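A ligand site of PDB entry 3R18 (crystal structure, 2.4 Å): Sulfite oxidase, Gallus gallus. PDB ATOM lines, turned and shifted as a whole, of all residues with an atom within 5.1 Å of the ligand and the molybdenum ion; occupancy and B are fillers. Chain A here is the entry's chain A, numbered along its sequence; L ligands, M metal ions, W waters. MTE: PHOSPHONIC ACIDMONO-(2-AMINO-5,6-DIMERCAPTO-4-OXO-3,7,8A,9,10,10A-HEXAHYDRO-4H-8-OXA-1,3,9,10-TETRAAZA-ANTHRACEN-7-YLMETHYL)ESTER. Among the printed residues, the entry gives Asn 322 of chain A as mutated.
S1' of the ligand sits close to NE of Arg 138, 3.8 Å away. N of His 140 is in hydrogen-bond range of O4 of the ligand (2.9 Å). ND1 of His 140 lies within hydrogen-bond range of O4 of the ligand (2.6 Å). The backbone carbonyl oxygen (O) of Ser 299 lies within hydrogen-bond range of a nitrogen (N8) of the ligand (3.0 Å). N2 of the ligand lies within hydrogen-bond range of O of Lys 301, at 3.0 Å. The guanidinium group of Arg 288 is in salt-bridge range of an oxygen (O3P) of the ligand. OD2 of Asp 244 is in hydrogen-bond range of N3 of the ligand (2.7 Å). An oxygen (O2P) of the ligand lies close to the backbone carbonyl oxygen (O) of Phe 136 (2.7 Å). ND1 of His 283 sits at hydrogen-bond distance from O3P of the ligand (2.7 Å). A nitrogen (N5) of the ligand lies within hydrogen-bond range of the backbone carbonyl oxygen (O) of Arg 138, at 3.4 Å. The backbone NH (N) of Lys 301 lies within hydrogen-bond range of a nitrogen (N1) of the ligand. An oxygen (O1P) of the ligand lies within salt-bridge range of the side-chain amino group (NZ) of Lys 301, at 2.8 Å. O1P of the ligand sits at hydrogen-bond distance from N of Arg 138 (3.1 Å).
The side-chain hydroxyl (OG1) of Thr 137 lies close to a ring nitrogen (NE2) of His 283, at 3.4 Å. OH of Tyr 252 is in hydrogen-bond range of O of Ala 297, at 2.6 Å. The backbone carbonyl oxygen of Tyr 252 is in hydrogen-bond range of the backbone NH of Gly 242 (2.8 Å). The side-chain amide nitrogen (ND2) of Asn 139 is in hydrogen-bond range of the side-chain carboxylate (OD1) of Asp 282. The backbone carbonyl oxygen (O) of Gln 184 is in hydrogen-bond range of the backbone NH (N) of Gly 296, 2.8 Å away. The backbone carbonyl oxygen (O) of Trp 302 is in hydrogen-bond range of the backbone NH (N) of Leu 243, 2.8 Å away. The backbone NH (N) of Gly 187 lies close to the side-chain sulfur (SG) of Cys 185 (3.5 Å). The side-chain amino group of Lys 301 sits at hydrogen-bond distance from the backbone carbonyl oxygen of Asp 282 (3.0 Å).
Residues that only touch the ligand: Phe 135, Thr 137, Asn 139, Gly 242, Tyr 252, Gly 296, Ala 297, Val 300 and Trp 302. Hydrophobic or aromatic side chains that line the ligand: Phe 135, Phe 136, His 140, Tyr 252, His 283, Ala 297 and Trp 302. 18 residues have an atom within 4 Å of the ligand: Phe 135, Phe 136, Thr 137, Arg 138, Asn 139, His 140, Cys 185, Gly 242, Asp 244, Tyr 252, His 283, Arg 288, Gly 296, Ala 297, Ser 299, Val 300, Lys 301 and Trp 302. The nearest printed residue that does not touch the ligand is Asp 282 (4.1 Å).
Merely in contact with the molybdenum ion: Ala 186 and Ala 297. Three residues have an atom within 4 Å of the molybdenum ion: Cys 185, Ala 186 and Ala 297. The nearest printed residue that does not touch the molybdenum ion is Arg 138 (4.3 Å).
Water W1 is bound to the molybdenum ion (1.7 Å). Water W2 binds the molybdenum ion, 2.0 Å away. The molybdenum ion is bound by S1' of the ligand, at 2.3 Å. The molybdenum ion is bound by S2' of the ligand, at 2.4 Å. SG of Cys 185 binds the molybdenum ion, at 2.5 Å.
Water W1 bridges N of Ala 186 (3.1 Å) and N of Ala 297 (3.1 Å). Water W3 lies within hydrogen-bond range of OD2 of Asp 244, N of Leu 141, N of His 140 and O4 of the ligand.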
ATOM      1  N   PHE A 135       7.698  19.285  29.102  1.00  0.00           N
ATOM      2  CA  PHE A 135       7.516  20.501  28.305  1.00  0.00           C
ATOM      3  C   PHE A 135       6.171  21.135  28.695  1.00  0.00           C
ATOM      4  O   PHE A 135       5.159  20.449  28.726  1.00  0.00           O
ATOM      5  CB  PHE A 135       7.541  20.148  26.818  1.00  0.00           C
ATOM      6  CG  PHE A 135       7.854  21.288  25.920  1.00  0.00           C
ATOM      7  CD1 PHE A 135       6.902  22.276  25.658  1.00  0.00           C
ATOM      8  CD2 PHE A 135       9.098  21.387  25.311  1.00  0.00           C
ATOM      9  CE1 PHE A 135       7.202  23.348  24.824  1.00  0.00           C
ATOM     10  CE2 PHE A 135       9.410  22.467  24.444  1.00  0.00           C
ATOM     11  CZ  PHE A 135       8.457  23.440  24.208  1.00  0.00           C
ATOM     12  N   PHE A 136       6.160  22.431  28.985  1.00  0.00           N
ATOM     13  CA  PHE A 136       4.931  23.101  29.427  1.00  0.00           C
ATOM     14  C   PHE A 136       3.830  22.926  28.394  1.00  0.00           C
ATOM     15  O   PHE A 136       4.104  22.848  27.186  1.00  0.00           O
ATOM     16  CB  PHE A 136       5.167  24.573  29.766  1.00  0.00           C
ATOM     17  CG  PHE A 136       4.980  25.538  28.607  1.00  0.00           C
ATOM     18  CD1 PHE A 136       6.008  25.768  27.693  1.00  0.00           C
ATOM     19  CD2 PHE A 136       3.789  26.252  28.456  1.00  0.00           C
ATOM     20  CE1 PHE A 136       5.846  26.666  26.632  1.00  0.00           C
ATOM     21  CE2 PHE A 136       3.622  27.163  27.391  1.00  0.00           C
ATOM     22  CZ  PHE A 136       4.648  27.357  26.467  1.00  0.00           C
ATOM     23  N   THR A 137       2.601  22.813  28.861  1.00  0.00           N
ATOM     24  CA  THR A 137       1.457  22.597  27.974  1.00  0.00           C
ATOM     25  C   THR A 137       0.451  23.712  28.183  1.00  0.00           C
ATOM     26  O   THR A 137       0.000  23.973  29.304  1.00  0.00           O
ATOM     27  CB  THR A 137       0.793  21.238  28.236  1.00  0.00           C
ATOM     28  OG1 THR A 137       1.753  20.210  28.005  1.00  0.00           O
ATOM     29  CG2 THR A 137      -0.390  21.003  27.290  1.00  0.00           C
ATOM     30  N   ARG A 138       0.093  24.350  27.075  1.00  0.00           N
ATOM     31  CA  ARG A 138      -0.926  25.379  27.036  1.00  0.00           C
ATOM     32  C   ARG A 138      -2.003  25.019  25.971  1.00  0.00           C
ATOM     33  O   ARG A 138      -1.728  25.072  24.773  1.00  0.00           O
ATOM     34  CB  ARG A 138      -0.258  26.722  26.727  1.00  0.00           C
ATOM     35  CG  ARG A 138      -1.011  27.948  27.217  1.00  0.00           C
ATOM     36  CD  ARG A 138      -2.185  28.255  26.315  1.00  0.00           C
ATOM     37  NE  ARG A 138      -2.916  29.436  26.769  1.00  0.00           N
ATOM     38  CZ  ARG A 138      -4.116  29.402  27.361  1.00  0.00           C
ATOM     39  NH1 ARG A 138      -4.719  28.234  27.586  1.00  0.00           N
ATOM     40  NH2 ARG A 138      -4.710  30.526  27.698  1.00  0.00           N
ATOM     41  N   ASN A 139      -3.201  24.621  26.429  1.00  0.00           N
ATOM     42  CA  ASN A 139      -4.329  24.294  25.549  1.00  0.00           C
ATOM     43  C   ASN A 139      -5.498  25.215  25.839  1.00  0.00           C
ATOM     44  O   ASN A 139      -5.805  25.475  27.015  1.00  0.00           O
ATOM     45  CB  ASN A 139      -4.809  22.854  25.780  1.00  0.00           C
ATOM     46  CG  ASN A 139      -3.735  21.802  25.546  1.00  0.00           C
ATOM     47  OD1 ASN A 139      -2.708  22.053  24.910  1.00  0.00           O
ATOM     48  ND2 ASN A 139      -3.984  20.600  26.057  1.00  0.00           N
ATOM     49  N   HIS A 140      -6.149  25.709  24.794  1.00  0.00           N
ATOM     50  CA  HIS A 140      -7.374  26.503  24.984  1.00  0.00           C
ATOM     51  C   HIS A 140      -8.589  25.575  24.981  1.00  0.00           C
ATOM     52  O   HIS A 140      -9.654  25.926  25.500  1.00  0.00           O
ATOM     53  CB  HIS A 140      -7.521  27.575  23.909  1.00  0.00           C
ATOM     54  CG  HIS A 140      -6.506  28.677  23.996  1.00  0.00           C
ATOM     55  ND1 HIS A 140      -5.206  28.539  23.554  1.00  0.00           N
ATOM     56  CD2 HIS A 140      -6.603  29.949  24.455  1.00  0.00           C
ATOM     57  CE1 HIS A 140      -4.546  29.658  23.751  1.00  0.00           C
ATOM     58  NE2 HIS A 140      -5.365  30.537  24.287  1.00  0.00           N
ATOM     59  N   LEU A 141      -8.419  24.386  24.416  1.00  0.00           N
ATOM     60  CA  LEU A 141      -9.561  23.548  24.041  1.00  0.00           C
ATOM     61  C   LEU A 141      -9.250  22.069  24.271  1.00  0.00           C
ATOM     62  O   LEU A 141      -8.111  21.737  24.608  1.00  0.00           O
ATOM     63  CB  LEU A 141      -9.887  23.782  22.551  1.00  0.00           C
ATOM     64  CG  LEU A 141     -10.383  25.202  22.187  1.00  0.00           C
ATOM     65  CD1 LEU A 141     -10.315  25.420  20.705  1.00  0.00           C
ATOM     66  CD2 LEU A 141     -11.819  25.527  22.755  1.00  0.00           C
ATOM     67  N   LEU A 183       9.922  27.750  23.202  1.00  0.00           N
ATOM     68  CA  LEU A 183       8.595  28.370  23.208  1.00  0.00           C
ATOM     69  C   LEU A 183       8.339  28.995  24.575  1.00  0.00           C
ATOM     70  O   LEU A 183       8.488  28.328  25.611  1.00  0.00           O
ATOM     71  CB  LEU A 183       7.490  27.379  22.813  1.00  0.00           C
ATOM     72  CG  LEU A 183       7.581  26.627  21.473  1.00  0.00           C
ATOM     73  CD1 LEU A 183       6.415  25.652  21.269  1.00  0.00           C
ATOM     74  CD2 LEU A 183       7.685  27.566  20.264  1.00  0.00           C
ATOM     75  N   GLN A 184       7.965  30.280  24.572  1.00  0.00           N
ATOM     76  CA  GLN A 184       7.519  30.968  25.775  1.00  0.00           C
ATOM     77  C   GLN A 184       6.110  31.485  25.553  1.00  0.00           C
ATOM     78  O   GLN A 184       5.817  32.116  24.537  1.00  0.00           O
ATOM     79  CB  GLN A 184       8.450  32.118  26.165  1.00  0.00           C
ATOM     80  CG  GLN A 184       8.070  32.732  27.514  1.00  0.00           C
ATOM     81  CD  GLN A 184       8.859  33.970  27.916  1.00  0.00           C
ATOM     82  OE1 GLN A 184       8.603  34.553  28.969  1.00  0.00           O
ATOM     83  NE2 GLN A 184       9.840  34.387  27.083  1.00  0.00           N
ATOM     84  N   CYS A 185       5.250  31.228  26.513  1.00  0.00           N
ATOM     85  CA  CYS A 185       3.917  31.775  26.499  1.00  0.00           C
ATOM     86  C   CYS A 185       3.958  33.254  26.913  1.00  0.00           C
ATOM     87  O   CYS A 185       4.692  33.621  27.830  1.00  0.00           O
ATOM     88  CB  CYS A 185       3.065  30.971  27.470  1.00  0.00           C
ATOM     89  SG  CYS A 185       1.336  31.365  27.419  1.00  0.00           S
ATOM     90  N   ALA A 186       3.150  34.102  26.256  1.00  0.00           N
ATOM     91  CA  ALA A 186       3.058  35.514  26.680  1.00  0.00           C
ATOM     92  C   ALA A 186       2.689  35.626  28.164  1.00  0.00           C
ATOM     93  O   ALA A 186       3.045  36.596  28.837  1.00  0.00           O
ATOM     94  CB  ALA A 186       2.047  36.263  25.837  1.00  0.00           C
ATOM     95  N   GLY A 187       1.988  34.608  28.659  1.00  0.00           N
ATOM     96  CA  GLY A 187       1.482  34.611  30.040  1.00  0.00           C
ATOM     97  C   GLY A 187       2.520  34.165  31.061  1.00  0.00           C
ATOM     98  O   GLY A 187       2.213  34.077  32.235  1.00  0.00           O
ATOM     99  N   TRP A 214      13.057  20.595  17.344  1.00  0.00           N
ATOM    100  CA  TRP A 214      11.926  20.344  16.480  1.00  0.00           C
ATOM    101  C   TRP A 214      12.389  19.879  15.111  1.00  0.00           C
ATOM    102  O   TRP A 214      13.444  20.302  14.643  1.00  0.00           O
ATOM    103  CB  TRP A 214      11.103  21.600  16.332  1.00  0.00           C
ATOM    104  CG  TRP A 214      10.734  22.265  17.633  1.00  0.00           C
ATOM    105  CD1 TRP A 214      11.363  23.329  18.236  1.00  0.00           C
ATOM    106  CD2 TRP A 214       9.632  21.919  18.495  1.00  0.00           C
ATOM    107  NE1 TRP A 214      10.718  23.658  19.402  1.00  0.00           N
ATOM    108  CE2 TRP A 214       9.657  22.816  19.575  1.00  0.00           C
ATOM    109  CE3 TRP A 214       8.635  20.943  18.432  1.00  0.00           C
ATOM    110  CZ2 TRP A 214       8.719  22.749  20.612  1.00  0.00           C
ATOM    111  CZ3 TRP A 214       7.701  20.882  19.457  1.00  0.00           C
ATOM    112  CH2 TRP A 214       7.745  21.789  20.525  1.00  0.00           C
ATOM    113  N   GLY A 242      -6.062  25.505  13.785  1.00  0.00           N
ATOM    114  CA  GLY A 242      -5.858  24.213  14.440  1.00  0.00           C
ATOM    115  C   GLY A 242      -7.082  23.345  14.258  1.00  0.00           C
ATOM    116  O   GLY A 242      -8.126  23.828  13.806  1.00  0.00           O
ATOM    117  N   LEU A 243      -6.955  22.063  14.597  1.00  0.00           N
ATOM    118  CA  LEU A 243      -8.087  21.129  14.561  1.00  0.00           C
ATOM    119  C   LEU A 243      -9.035  21.318  15.746  1.00  0.00           C
ATOM    120  O   LEU A 243     -10.174  20.864  15.710  1.00  0.00           O
ATOM    121  CB  LEU A 243      -7.591  19.658  14.499  1.00  0.00           C
ATOM    122  CG  LEU A 243      -7.135  19.126  13.129  1.00  0.00           C
ATOM    123  CD1 LEU A 243      -6.411  17.790  13.264  1.00  0.00           C
ATOM    124  CD2 LEU A 243      -8.317  19.015  12.131  1.00  0.00           C
ATOM    125  N   ASP A 244      -8.561  22.014  16.774  1.00  0.00           N
ATOM    126  CA  ASP A 244      -9.369  22.318  17.965  1.00  0.00           C
ATOM    127  C   ASP A 244     -10.269  23.555  17.773  1.00  0.00           C
ATOM    128  O   ASP A 244      -9.809  24.602  17.353  1.00  0.00           O
ATOM    129  CB  ASP A 244      -8.476  22.482  19.195  1.00  0.00           C
ATOM    130  CG  ASP A 244      -7.322  23.441  18.950  1.00  0.00           C
ATOM    131  OD1 ASP A 244      -6.891  23.603  17.772  1.00  0.00           O
ATOM    132  OD2 ASP A 244      -6.815  24.015  19.936  1.00  0.00           O
ATOM    133  N   TYR A 252      -8.951  27.338  16.812  1.00  0.00           N
ATOM    134  CA  TYR A 252      -7.842  28.147  17.268  1.00  0.00           C
ATOM    135  C   TYR A 252      -7.105  28.658  16.034  1.00  0.00           C
ATOM    136  O   TYR A 252      -6.830  27.879  15.100  1.00  0.00           O
ATOM    137  CB  TYR A 252      -6.900  27.387  18.194  1.00  0.00           C
ATOM    138  CG  TYR A 252      -5.797  28.284  18.704  1.00  0.00           C
ATOM    139  CD1 TYR A 252      -6.027  29.182  19.772  1.00  0.00           C
ATOM    140  CD2 TYR A 252      -4.549  28.307  18.078  1.00  0.00           C
ATOM    141  CE1 TYR A 252      -5.021  30.029  20.216  1.00  0.00           C
ATOM    142  CE2 TYR A 252      -3.541  29.148  18.503  1.00  0.00           C
ATOM    143  CZ  TYR A 252      -3.779  30.004  19.573  1.00  0.00           C
ATOM    144  OH  TYR A 252      -2.743  30.806  19.993  1.00  0.00           O
ATOM    145  N   ASP A 282      -0.594  16.342  23.261  1.00  0.00           N
ATOM    146  CA  ASP A 282      -0.637  17.647  23.936  1.00  0.00           C
ATOM    147  C   ASP A 282       0.162  18.733  23.205  1.00  0.00           C
ATOM    148  O   ASP A 282      -0.110  19.928  23.358  1.00  0.00           O
ATOM    149  CB  ASP A 282      -0.136  17.554  25.385  1.00  0.00           C
ATOM    150  CG  ASP A 282      -1.266  17.366  26.382  1.00  0.00           C
ATOM    151  OD1 ASP A 282      -2.435  17.678  26.038  1.00  0.00           O
ATOM    152  OD2 ASP A 282      -0.995  16.895  27.512  1.00  0.00           O
ATOM    153  N   HIS A 283       1.156  18.309  22.419  1.00  0.00           N
ATOM    154  CA  HIS A 283       2.013  19.249  21.731  1.00  0.00           C
ATOM    155  C   HIS A 283       1.768  19.335  20.233  1.00  0.00           C
ATOM    156  O   HIS A 283       2.599  19.868  19.497  1.00  0.00           O
ATOM    157  CB  HIS A 283       3.478  19.038  22.110  1.00  0.00           C
ATOM    158  CG  HIS A 283       3.733  19.206  23.578  1.00  0.00           C
ATOM    159  ND1 HIS A 283       3.773  20.439  24.189  1.00  0.00           N
ATOM    160  CD2 HIS A 283       3.893  18.287  24.560  1.00  0.00           C
ATOM    161  CE1 HIS A 283       3.965  20.277  25.485  1.00  0.00           C
ATOM    162  NE2 HIS A 283       4.036  18.977  25.741  1.00  0.00           N
ATOM    163  N   ARG A 288       2.389  20.654  13.978  1.00  0.00           N
ATOM    164  CA  ARG A 288       2.274  21.989  14.543  1.00  0.00           C
ATOM    165  C   ARG A 288       3.174  22.927  13.764  1.00  0.00           C
ATOM    166  O   ARG A 288       4.180  22.483  13.175  1.00  0.00           O
ATOM    167  CB  ARG A 288       2.680  21.979  16.029  1.00  0.00           C
ATOM    168  CG  ARG A 288       4.179  22.050  16.277  1.00  0.00           C
ATOM    169  CD  ARG A 288       4.510  22.258  17.738  1.00  0.00           C
ATOM    170  NE  ARG A 288       3.979  23.515  18.249  1.00  0.00           N
ATOM    171  CZ  ARG A 288       3.823  23.801  19.546  1.00  0.00           C
ATOM    172  NH1 ARG A 288       4.163  22.895  20.456  1.00  0.00           N
ATOM    173  NH2 ARG A 288       3.309  24.977  19.926  1.00  0.00           N
ATOM    174  N   GLY A 296       4.668  31.923  21.963  1.00  0.00           N
ATOM    175  CA  GLY A 296       4.094  30.576  21.775  1.00  0.00           C
ATOM    176  C   GLY A 296       2.747  30.553  21.071  1.00  0.00           C
ATOM    177  O   GLY A 296       2.474  29.637  20.292  1.00  0.00           O
ATOM    178  N   ALA A 297       1.905  31.544  21.346  1.00  0.00           N
ATOM    179  CA  ALA A 297       0.593  31.726  20.694  1.00  0.00           C
ATOM    180  C   ALA A 297       0.550  31.458  19.183  1.00  0.00           C
ATOM    181  O   ALA A 297      -0.464  30.979  18.669  1.00  0.00           O
ATOM    182  CB  ALA A 297       0.043  33.151  20.989  1.00  0.00           C
ATOM    183  N   SER A 299       2.633  29.491  17.406  1.00  0.00           N
ATOM    184  CA  SER A 299       3.042  28.142  17.042  1.00  0.00           C
ATOM    185  C   SER A 299       1.832  27.184  17.102  1.00  0.00           C
ATOM    186  O   SER A 299       1.687  26.410  18.042  1.00  0.00           O
ATOM    187  CB  SER A 299       4.200  27.661  17.916  1.00  0.00           C
ATOM    188  OG  SER A 299       5.419  28.288  17.522  1.00  0.00           O
ATOM    189  N   VAL A 300       0.968  27.277  16.097  1.00  0.00           N
ATOM    190  CA  VAL A 300      -0.336  26.611  16.116  1.00  0.00           C
ATOM    191  C   VAL A 300      -0.259  25.077  16.090  1.00  0.00           C
ATOM    192  O   VAL A 300       0.308  24.472  15.156  1.00  0.00           O
ATOM    193  CB  VAL A 300      -1.226  27.141  14.964  1.00  0.00           C
ATOM    194  CG1 VAL A 300      -2.545  26.334  14.870  1.00  0.00           C
ATOM    195  CG2 VAL A 300      -1.490  28.641  15.143  1.00  0.00           C
ATOM    196  N   LYS A 301      -0.819  24.452  17.123  1.00  0.00           N
ATOM    197  CA  LYS A 301      -0.822  22.987  17.235  1.00  0.00           C
ATOM    198  C   LYS A 301      -1.961  22.346  16.416  1.00  0.00           C
ATOM    199  O   LYS A 301      -2.900  23.051  16.037  1.00  0.00           O
ATOM    200  CB  LYS A 301      -0.922  22.597  18.708  1.00  0.00           C
ATOM    201  CG  LYS A 301       0.309  22.988  19.512  1.00  0.00           C
ATOM    202  CD  LYS A 301       0.226  22.484  20.939  1.00  0.00           C
ATOM    203  CE  LYS A 301      -0.586  23.410  21.861  1.00  0.00           C
ATOM    204  NZ  LYS A 301      -0.740  22.825  23.245  1.00  0.00           N
ATOM    205  N   TRP A 302      -1.851  21.045  16.125  1.00  0.00           N
ATOM    206  CA  TRP A 302      -2.919  20.296  15.421  1.00  0.00           C
ATOM    207  C   TRP A 302      -3.325  20.970  14.107  1.00  0.00           C
ATOM    208  O   TRP A 302      -4.518  21.069  13.788  1.00  0.00           O
ATOM    209  CB  TRP A 302      -4.136  20.072  16.338  1.00  0.00           C
ATOM    210  CG  TRP A 302      -3.758  19.568  17.711  1.00  0.00           C
ATOM    211  CD1 TRP A 302      -3.248  18.344  18.012  1.00  0.00           C
ATOM    212  CD2 TRP A 302      -3.786  20.305  18.945  1.00  0.00           C
ATOM    213  NE1 TRP A 302      -2.969  18.257  19.365  1.00  0.00           N
ATOM    214  CE2 TRP A 302      -3.302  19.446  19.957  1.00  0.00           C
ATOM    215  CE3 TRP A 302      -4.198  21.597  19.307  1.00  0.00           C
ATOM    216  CZ2 TRP A 302      -3.200  19.831  21.298  1.00  0.00           C
ATOM    217  CZ3 TRP A 302      -4.118  21.981  20.645  1.00  0.00           C
ATOM    218  CH2 TRP A 302      -3.604  21.098  21.626  1.00  0.00           C
ATOM    219  N   ASN A 322      -3.081  38.296  24.162  1.00  0.00           N
ATOM    220  CA  ASN A 322      -1.652  38.430  23.928  1.00  0.00           C
ATOM    221  C   ASN A 322      -1.295  39.710  23.157  1.00  0.00           C
ATOM    222  O   ASN A 322      -0.661  39.683  22.091  1.00  0.00           O
ATOM    223  CB  ASN A 322      -1.122  37.146  23.278  1.00  0.00           C
ATOM    224  CG  ASN A 322      -1.295  35.927  24.192  1.00  0.00           C
ATOM    225  OD1 ASN A 322      -0.970  35.981  25.387  1.00  0.00           O
ATOM    226  ND2 ASN A 322      -1.824  34.836  23.639  1.00  0.00           N
HETATM  227  N1  MTE L   1      -2.555  25.741  18.985  1.00  0.00           N
HETATM  228  C2  MTE L   1      -3.826  25.290  19.084  1.00  0.00           C
HETATM  229  N2  MTE L   1      -4.380  24.651  18.030  1.00  0.00           N
HETATM  230  N3  MTE L   1      -4.562  25.467  20.207  1.00  0.00           N
HETATM  231  C4  MTE L   1      -4.073  26.101  21.288  1.00  0.00           C
HETATM  232  O4  MTE L   1      -4.782  26.255  22.295  1.00  0.00           O
HETATM  233  N5  MTE L   1      -2.087  27.313  22.270  1.00  0.00           N
HETATM  234  C6  MTE L   1      -1.075  28.299  21.865  1.00  0.00           C
HETATM  235  C7  MTE L   1      -0.033  27.617  20.957  1.00  0.00           C
HETATM  236  N8  MTE L   1      -0.663  26.851  19.886  1.00  0.00           N
HETATM  237  C9  MTE L   1      -2.684  26.627  21.259  1.00  0.00           C
HETATM  238  C10 MTE L   1      -1.939  26.394  19.997  1.00  0.00           C
HETATM  239  C1' MTE L   1      -0.329  29.017  22.974  1.00  0.00           C
HETATM  240  S1' MTE L   1      -1.054  30.413  23.622  1.00  0.00           S
HETATM  241  C2' MTE L   1       0.879  28.598  23.378  1.00  0.00           C
HETATM  242  S2' MTE L   1       1.742  29.396  24.617  1.00  0.00           S
HETATM  243  C3' MTE L   1       1.577  27.411  22.721  1.00  0.00           C
HETATM  244  O3' MTE L   1       0.760  26.737  21.761  1.00  0.00           O
HETATM  245  C4' MTE L   1       2.029  26.386  23.786  1.00  0.00           C
HETATM  246  O4' MTE L   1       2.541  25.220  23.149  1.00  0.00           O
HETATM  247  P   MTE L   1       2.925  23.900  23.988  1.00  0.00           P
HETATM  248  O1P MTE L   1       1.607  23.399  24.564  1.00  0.00           O
HETATM  249  O2P MTE L   1       3.889  24.451  24.990  1.00  0.00           O
HETATM  250  O3P MTE L   1       3.533  22.908  23.037  1.00  0.00           O
HETATM  251 MO    MO M   1       0.496  31.402  25.071  1.00  0.00          MO
HETATM  252  O   HOH W   1       1.383  32.637  24.247  1.00  0.00           O
HETATM  253  O   HOH W   2      -1.217  32.086  25.782  1.00  0.00           O
HETATM  254  O   HOH W   3      -6.331  23.171  22.677  1.00  0.00           O
